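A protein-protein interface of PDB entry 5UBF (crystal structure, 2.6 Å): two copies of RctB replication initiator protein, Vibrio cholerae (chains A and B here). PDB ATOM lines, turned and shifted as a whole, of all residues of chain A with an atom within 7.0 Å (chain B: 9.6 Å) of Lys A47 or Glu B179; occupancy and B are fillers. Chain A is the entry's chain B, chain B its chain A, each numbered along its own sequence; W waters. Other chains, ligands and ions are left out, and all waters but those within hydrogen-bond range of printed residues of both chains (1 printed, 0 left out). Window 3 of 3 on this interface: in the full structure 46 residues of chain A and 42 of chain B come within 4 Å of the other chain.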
ATOM      1  N   ALA A  35       5.016 -13.715  -1.462  1.00  0.00           N
ATOM      2  CA  ALA A  35       6.040 -12.718  -1.169  1.00  0.00           C
ATOM      3  C   ALA A  35       6.189 -12.491   0.330  1.00  0.00           C
ATOM      4  O   ALA A  35       6.482 -11.375   0.768  1.00  0.00           O
ATOM      5  CB  ALA A  35       5.737 -11.397  -1.873  1.00  0.00           C
ATOM      6  N   LYS A  43      13.251 -10.196   9.130  1.00  0.00           N
ATOM      7  CA  LYS A  43      13.948  -9.399   8.133  1.00  0.00           C
ATOM      8  C   LYS A  43      13.076  -8.218   7.734  1.00  0.00           C
ATOM      9  O   LYS A  43      11.870  -8.192   7.995  1.00  0.00           O
ATOM     10  CB  LYS A  43      14.315 -10.240   6.901  1.00  0.00           C
ATOM     11  CG  LYS A  43      13.134 -10.960   6.270  1.00  0.00           C
ATOM     12  CD  LYS A  43      13.590 -12.096   5.365  1.00  0.00           C
ATOM     13  CE  LYS A  43      14.536 -11.604   4.283  1.00  0.00           C
ATOM     14  NZ  LYS A  43      14.939 -12.698   3.357  1.00  0.00           N
ATOM     15  N   TYR A  45      13.377  -6.692   4.421  1.00  0.00           N
ATOM     16  CA  TYR A  45      13.300  -6.540   2.976  1.00  0.00           C
ATOM     17  C   TYR A  45      13.355  -7.916   2.328  1.00  0.00           C
ATOM     18  O   TYR A  45      14.126  -8.779   2.755  1.00  0.00           O
ATOM     19  CB  TYR A  45      14.434  -5.658   2.441  1.00  0.00           C
ATOM     20  CG  TYR A  45      14.465  -5.563   0.931  1.00  0.00           C
ATOM     21  CD1 TYR A  45      13.683  -4.633   0.259  1.00  0.00           C
ATOM     22  CD2 TYR A  45      15.276  -6.404   0.178  1.00  0.00           C
ATOM     23  CE1 TYR A  45      13.706  -4.544  -1.121  1.00  0.00           C
ATOM     24  CE2 TYR A  45      15.306  -6.323  -1.200  1.00  0.00           C
ATOM     25  CZ  TYR A  45      14.520  -5.393  -1.845  1.00  0.00           C
ATOM     26  OH  TYR A  45      14.551  -5.311  -3.218  1.00  0.00           O
ATOM     27  N   GLN A  46      12.540  -8.104   1.293  1.00  0.00           N
ATOM     28  CA  GLN A  46      12.534  -9.344   0.528  1.00  0.00           C
ATOM     29  C   GLN A  46      12.093  -9.034  -0.894  1.00  0.00           C
ATOM     30  O   GLN A  46      11.064  -8.386  -1.098  1.00  0.00           O
ATOM     31  CB  GLN A  46      11.608 -10.388   1.161  1.00  0.00           C
ATOM     32  CG  GLN A  46      11.553 -11.707   0.407  1.00  0.00           C
ATOM     33  CD  GLN A  46      10.790 -12.776   1.162  1.00  0.00           C
ATOM     34  OE1 GLN A  46      11.157 -13.146   2.277  1.00  0.00           O
ATOM     35  NE2 GLN A  46       9.717 -13.273   0.560  1.00  0.00           N
ATOM     36  N   LYS A  47      12.875  -9.494  -1.868  1.00  0.00           N
ATOM     37  CA  LYS A  47      12.614  -9.251  -3.284  1.00  0.00           C
ATOM     38  C   LYS A  47      12.338 -10.591  -3.953  1.00  0.00           C
ATOM     39  O   LYS A  47      13.225 -11.447  -4.030  1.00  0.00           O
ATOM     40  CB  LYS A  47      13.797  -8.539  -3.939  1.00  0.00           C
ATOM     41  CG  LYS A  47      13.609  -8.226  -5.411  1.00  0.00           C
ATOM     42  CD  LYS A  47      14.846  -7.554  -5.987  1.00  0.00           C
ATOM     43  CE  LYS A  47      16.081  -8.424  -5.799  1.00  0.00           C
ATOM     44  NZ  LYS A  47      17.304  -7.791  -6.368  1.00  0.00           N
ATOM     45  N   SER A  48      11.110 -10.775  -4.432  1.00  0.00           N
ATOM     46  CA  SER A  48      10.695 -12.024  -5.049  1.00  0.00           C
ATOM     47  C   SER A  48      10.288 -11.791  -6.497  1.00  0.00           C
ATOM     48  O   SER A  48       9.751 -10.737  -6.849  1.00  0.00           O
ATOM     49  CB  SER A  48       9.533 -12.664  -4.278  1.00  0.00           C
ATOM     50  OG  SER A  48       9.896 -12.920  -2.931  1.00  0.00           O
ATOM     51  N   MET A  49      10.554 -12.788  -7.334  1.00  0.00           N
ATOM     52  CA  MET A  49      10.172 -12.740  -8.740  1.00  0.00           C
ATOM     53  C   MET A  49       8.872 -13.508  -8.946  1.00  0.00           C
ATOM     54  O   MET A  49       8.761 -14.667  -8.548  1.00  0.00           O
ATOM     55  CB  MET A  49      11.280 -13.320  -9.621  1.00  0.00           C
ATOM     56  CG  MET A  49      11.102 -13.065 -11.109  1.00  0.00           C
ATOM     57  SD  MET A  49      11.517 -11.230 -11.630  1.00  0.00           S
ATOM     58  CE  MET A  49      11.340 -11.425 -13.563  1.00  0.00           C
ATOM     59  N   VAL A  58       8.291  -7.970 -10.385  1.00  0.00           N
ATOM     60  CA  VAL A  58       9.123  -8.043  -9.189  1.00  0.00           C
ATOM     61  C   VAL A  58       8.297  -7.524  -8.022  1.00  0.00           C
ATOM     62  O   VAL A  58       7.853  -6.370  -8.034  1.00  0.00           O
ATOM     63  CB  VAL A  58      10.420  -7.237  -9.345  1.00  0.00           C
ATOM     64  CG1 VAL A  58      11.234  -7.292  -8.061  1.00  0.00           C
ATOM     65  CG2 VAL A  58      11.233  -7.756 -10.520  1.00  0.00           C
ATOM     66  N   ILE A  59       8.088  -8.369  -7.018  1.00  0.00           N
ATOM     67  CA  ILE A  59       7.333  -7.996  -5.827  1.00  0.00           C
ATOM     68  C   ILE A  59       8.318  -7.790  -4.683  1.00  0.00           C
ATOM     69  O   ILE A  59       9.088  -8.696  -4.340  1.00  0.00           O
ATOM     70  CB  ILE A  59       6.264  -9.042  -5.473  1.00  0.00           C
ATOM     71  CG1 ILE A  59       5.617  -8.706  -4.129  1.00  0.00           C
ATOM     72  CG2 ILE A  59       6.841 -10.454  -5.477  1.00  0.00           C
ATOM     73  CD1 ILE A  59       4.834  -7.415  -4.136  1.00  0.00           C
ATOM     74  N   GLU A  60       8.306  -6.591  -4.109  1.00  0.00           N
ATOM     75  CA  GLU A  60       9.134  -6.251  -2.962  1.00  0.00           C
ATOM     76  C   GLU A  60       8.270  -6.175  -1.712  1.00  0.00           C
ATOM     77  O   GLU A  60       7.125  -5.714  -1.761  1.00  0.00           O
ATOM     78  CB  GLU A  60       9.858  -4.918  -3.167  1.00  0.00           C
ATOM     79  CG  GLU A  60      10.763  -4.865  -4.382  1.00  0.00           C
ATOM     80  CD  GLU A  60      11.487  -3.538  -4.503  1.00  0.00           C
ATOM     81  OE1 GLU A  60      12.684  -3.474  -4.149  1.00  0.00           O
ATOM     82  OE2 GLU A  60      10.854  -2.554  -4.938  1.00  0.00           O
ATOM     83  N   THR A  61       8.829  -6.630  -0.594  1.00  0.00           N
ATOM     84  CA  THR A  61       8.167  -6.589   0.704  1.00  0.00           C
ATOM     85  C   THR A  61       9.128  -5.948   1.689  1.00  0.00           C
ATOM     86  O   THR A  61      10.226  -6.468   1.912  1.00  0.00           O
ATOM     87  CB  THR A  61       7.774  -7.994   1.169  1.00  0.00           C
ATOM     88  OG1 THR A  61       6.832  -8.558   0.249  1.00  0.00           O
ATOM     89  CG2 THR A  61       7.156  -7.947   2.555  1.00  0.00           C
ATOM     90  N   ALA B 176      12.102   2.139 -17.588  1.00  0.00           N
ATOM     91  CA  ALA B 176      11.959   0.797 -17.051  1.00  0.00           C
ATOM     92  C   ALA B 176      12.420   0.743 -15.595  1.00  0.00           C
ATOM     93  O   ALA B 176      13.242   1.558 -15.166  1.00  0.00           O
ATOM     94  CB  ALA B 176      12.763  -0.196 -17.884  1.00  0.00           C
ATOM     95  N   PRO B 177      11.890  -0.197 -14.812  1.00  0.00           N
ATOM     96  CA  PRO B 177      12.385  -0.377 -13.440  1.00  0.00           C
ATOM     97  C   PRO B 177      13.861  -0.752 -13.438  1.00  0.00           C
ATOM     98  O   PRO B 177      14.288  -1.671 -14.141  1.00  0.00           O
ATOM     99  CB  PRO B 177      11.511  -1.511 -12.893  1.00  0.00           C
ATOM    100  CG  PRO B 177      10.271  -1.466 -13.722  1.00  0.00           C
ATOM    101  CD  PRO B 177      10.717  -1.043 -15.091  1.00  0.00           C
ATOM    102  N   VAL B 178      14.640  -0.031 -12.637  1.00  0.00           N
ATOM    103  CA  VAL B 178      16.087  -0.195 -12.574  1.00  0.00           C
ATOM    104  C   VAL B 178      16.453  -0.799 -11.226  1.00  0.00           C
ATOM    105  O   VAL B 178      16.024  -0.301 -10.178  1.00  0.00           O
ATOM    106  CB  VAL B 178      16.815   1.144 -12.789  1.00  0.00           C
ATOM    107  CG1 VAL B 178      18.319   0.959 -12.662  1.00  0.00           C
ATOM    108  CG2 VAL B 178      16.457   1.730 -14.147  1.00  0.00           C
ATOM    109  N   GLU B 179      17.243  -1.870 -11.254  1.00  0.00           N
ATOM    110  CA  GLU B 179      17.775  -2.481 -10.041  1.00  0.00           C
ATOM    111  C   GLU B 179      19.068  -1.763  -9.673  1.00  0.00           C
ATOM    112  O   GLU B 179      20.087  -1.914 -10.354  1.00  0.00           O
ATOM    113  CB  GLU B 179      18.009  -3.976 -10.241  1.00  0.00           C
ATOM    114  CG  GLU B 179      18.535  -4.688  -9.004  1.00  0.00           C
ATOM    115  CD  GLU B 179      18.635  -6.190  -9.190  1.00  0.00           C
ATOM    116  OE1 GLU B 179      18.477  -6.661 -10.335  1.00  0.00           O
ATOM    117  OE2 GLU B 179      18.870  -6.900  -8.188  1.00  0.00           O
ATOM    118  N   GLY B 180      19.025  -0.981  -8.598  1.00  0.00           N
ATOM    119  CA  GLY B 180      20.162  -0.185  -8.192  1.00  0.00           C
ATOM    120  C   GLY B 180      21.309  -1.024  -7.658  1.00  0.00           C
ATOM    121  O   GLY B 180      21.287  -2.256  -7.644  1.00  0.00           O
ATOM    122  N   SER B 181      22.347  -0.319  -7.201  1.00  0.00           N
ATOM    123  CA  SER B 181      23.533  -0.979  -6.673  1.00  0.00           C
ATOM    124  C   SER B 181      23.256  -1.724  -5.373  1.00  0.00           C
ATOM    125  O   SER B 181      23.999  -2.654  -5.037  1.00  0.00           O
ATOM    126  CB  SER B 181      24.652   0.041  -6.459  1.00  0.00           C
ATOM    127  OG  SER B 181      24.226   1.098  -5.615  1.00  0.00           O
ATOM    128  N   ASP B 182      22.213  -1.345  -4.641  1.00  0.00           N
ATOM    129  CA  ASP B 182      21.843  -2.018  -3.403  1.00  0.00           C
ATOM    130  C   ASP B 182      20.956  -3.235  -3.632  1.00  0.00           C
ATOM    131  O   ASP B 182      20.538  -3.871  -2.658  1.00  0.00           O
ATOM    132  CB  ASP B 182      21.142  -1.036  -2.455  1.00  0.00           C
ATOM    133  CG  ASP B 182      19.968  -0.325  -3.108  1.00  0.00           C
ATOM    134  OD1 ASP B 182      19.704  -0.573  -4.304  1.00  0.00           O
ATOM    135  OD2 ASP B 182      19.308   0.485  -2.422  1.00  0.00           O
ATOM    136  N   GLY B 183      20.664  -3.576  -4.885  1.00  0.00           N
ATOM    137  CA  GLY B 183      19.827  -4.718  -5.187  1.00  0.00           C
ATOM    138  C   GLY B 183      18.340  -4.478  -5.059  1.00  0.00           C
ATOM    139  O   GLY B 183      17.566  -5.439  -5.139  1.00  0.00           O
ATOM    140  N   GLU B 184      17.915  -3.233  -4.865  1.00  0.00           N
ATOM    141  CA  GLU B 184      16.510  -2.897  -4.701  1.00  0.00           C
ATOM    142  C   GLU B 184      16.004  -2.146  -5.926  1.00  0.00           C
ATOM    143  O   GLU B 184      16.765  -1.463  -6.618  1.00  0.00           O
ATOM    144  CB  GLU B 184      16.289  -2.057  -3.440  1.00  0.00           C
ATOM    145  CG  GLU B 184      16.728  -2.752  -2.162  1.00  0.00           C
ATOM    146  CD  GLU B 184      16.439  -1.937  -0.915  1.00  0.00           C
ATOM    147  OE1 GLU B 184      15.908  -0.814  -1.044  1.00  0.00           O
ATOM    148  OE2 GLU B 184      16.744  -2.424   0.195  1.00  0.00           O
ATOM    149  N   ILE B 185      14.707  -2.280  -6.186  1.00  0.00           N
ATOM    150  CA  ILE B 185      14.098  -1.707  -7.381  1.00  0.00           C
ATOM    151  C   ILE B 185      13.935  -0.205  -7.194  1.00  0.00           C
ATOM    152  O   ILE B 185      13.428   0.256  -6.166  1.00  0.00           O
ATOM    153  CB  ILE B 185      12.748  -2.377  -7.678  1.00  0.00           C
ATOM    154  CG1 ILE B 185      12.931  -3.887  -7.847  1.00  0.00           C
ATOM    155  CG2 ILE B 185      12.108  -1.769  -8.917  1.00  0.00           C
ATOM    156  CD1 ILE B 185      13.918  -4.261  -8.927  1.00  0.00           C
ATOM    157  N   ARG B 186      14.368   0.562  -8.192  1.00  0.00           N
ATOM    158  CA  ARG B 186      14.200   2.008  -8.212  1.00  0.00           C
ATOM    159  C   ARG B 186      13.383   2.390  -9.437  1.00  0.00           C
ATOM    160  O   ARG B 186      13.734   2.017 -10.562  1.00  0.00           O
ATOM    161  CB  ARG B 186      15.553   2.724  -8.229  1.00  0.00           C
ATOM    162  CG  ARG B 186      15.445   4.238  -8.177  1.00  0.00           C
ATOM    163  CD  ARG B 186      16.809   4.887  -8.016  1.00  0.00           C
ATOM    164  NE  ARG B 186      16.707   6.333  -7.845  1.00  0.00           N
ATOM    165  CZ  ARG B 186      16.546   6.937  -6.671  1.00  0.00           C
ATOM    166  NH1 ARG B 186      16.468   6.218  -5.560  1.00  0.00           N
ATOM    167  NH2 ARG B 186      16.463   8.259  -6.609  1.00  0.00           N
ATOM    168  N   ILE B 187      12.299   3.126  -9.218  1.00  0.00           N
ATOM    169  CA  ILE B 187      11.394   3.512 -10.288  1.00  0.00           C
ATOM    170  C   ILE B 187      11.458   5.022 -10.477  1.00  0.00           C
ATOM    171  O   ILE B 187      11.900   5.773  -9.602  1.00  0.00           O
ATOM    172  CB  ILE B 187       9.948   3.052 -10.014  1.00  0.00           C
ATOM    173  CG1 ILE B 187       9.376   3.771  -8.794  1.00  0.00           C
ATOM    174  CG2 ILE B 187       9.901   1.547  -9.808  1.00  0.00           C
ATOM    175  CD1 ILE B 187       7.973   3.329  -8.430  1.00  0.00           C
HETATM  176  O   HOH W   1      11.531  -0.195  -4.035  1.00  0.00           O
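OE2 of Glu B179 is in salt-bridge range of NZ of Lys A47 (2.6 Å). The side-chain amino group (NZ) of Lys A47 is in hydrogen-bond range of the backbone carbonyl oxygen (O) of Gly B183, 2.7 Å away. The side-chain carboxylate (OE1) of Glu A60 lies within hydrogen-bond range of the backbone NH (N) of Ile B185, at 3.1 Å.
The side-chain carboxylate (OD1) of Asp B182 lies within hydrogen-bond range of the backbone NH (N) of Glu B184. The side-chain carboxylate (OE1) of Glu A60 sits at hydrogen-bond distance from the side-chain hydroxyl (OH) of Tyr A45 (2.8 Å).
Among the printed residues, merely in contact across the chains: Tyr A45 with Glu B184, Tyr A45 with Gly B183, Val A58 with Ile B185 and Glu A60 with Glu B184.
Of chain A, only Lys A47 comes within 4 Å of Glu B179. No residue of chain B comes within 4 Å of Ser A48. Printed residues of chain B within 4 Å of Tyr A45: Gly B183 (3.6 Å) and Glu B184 (3.4 Å). Printed residues of chain B within 4 Å of Val A58: Ile B185. Of the printed residues of chain B, Glu A60 touches Glu B184 and Ile B185. Ile A59 touches none of the printed residues of chain B. Ala B176 touches none of the printed residues of chain A. The nearest residue of chain A that does not touch Glu B179 is Tyr A45 (6.8 Å). The nearest printed residue of chain A that does not touch Ile B185 is Tyr A45 (4.2 Å).
Of the 12 printed residues of chain B, 4 touch a printed residue of chain A. Hydrophobic or aromatic side chains of chain B that line the printed part of chain A: Ile B185. Printed residues of chain A that touch a printed residue of chain B: Tyr A45, Lys A47, Val A58 and Glu A60. Among the printed residues, Asp or Glu carboxylates within 4 Å of a Lys or Arg side-chain nitrogen of the other chain: Lys A47 with Glu B179.
No position is printed for both chains. Of the 7 pairs that touch across the chains among the printed residues, none has its exchanged pair printed and touching as well.
Water W1 bridges the side-chain carboxylate of Glu A60 (2.6 Å) and the backbone carbonyl oxygen of Ile B185 (2.9 Å).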
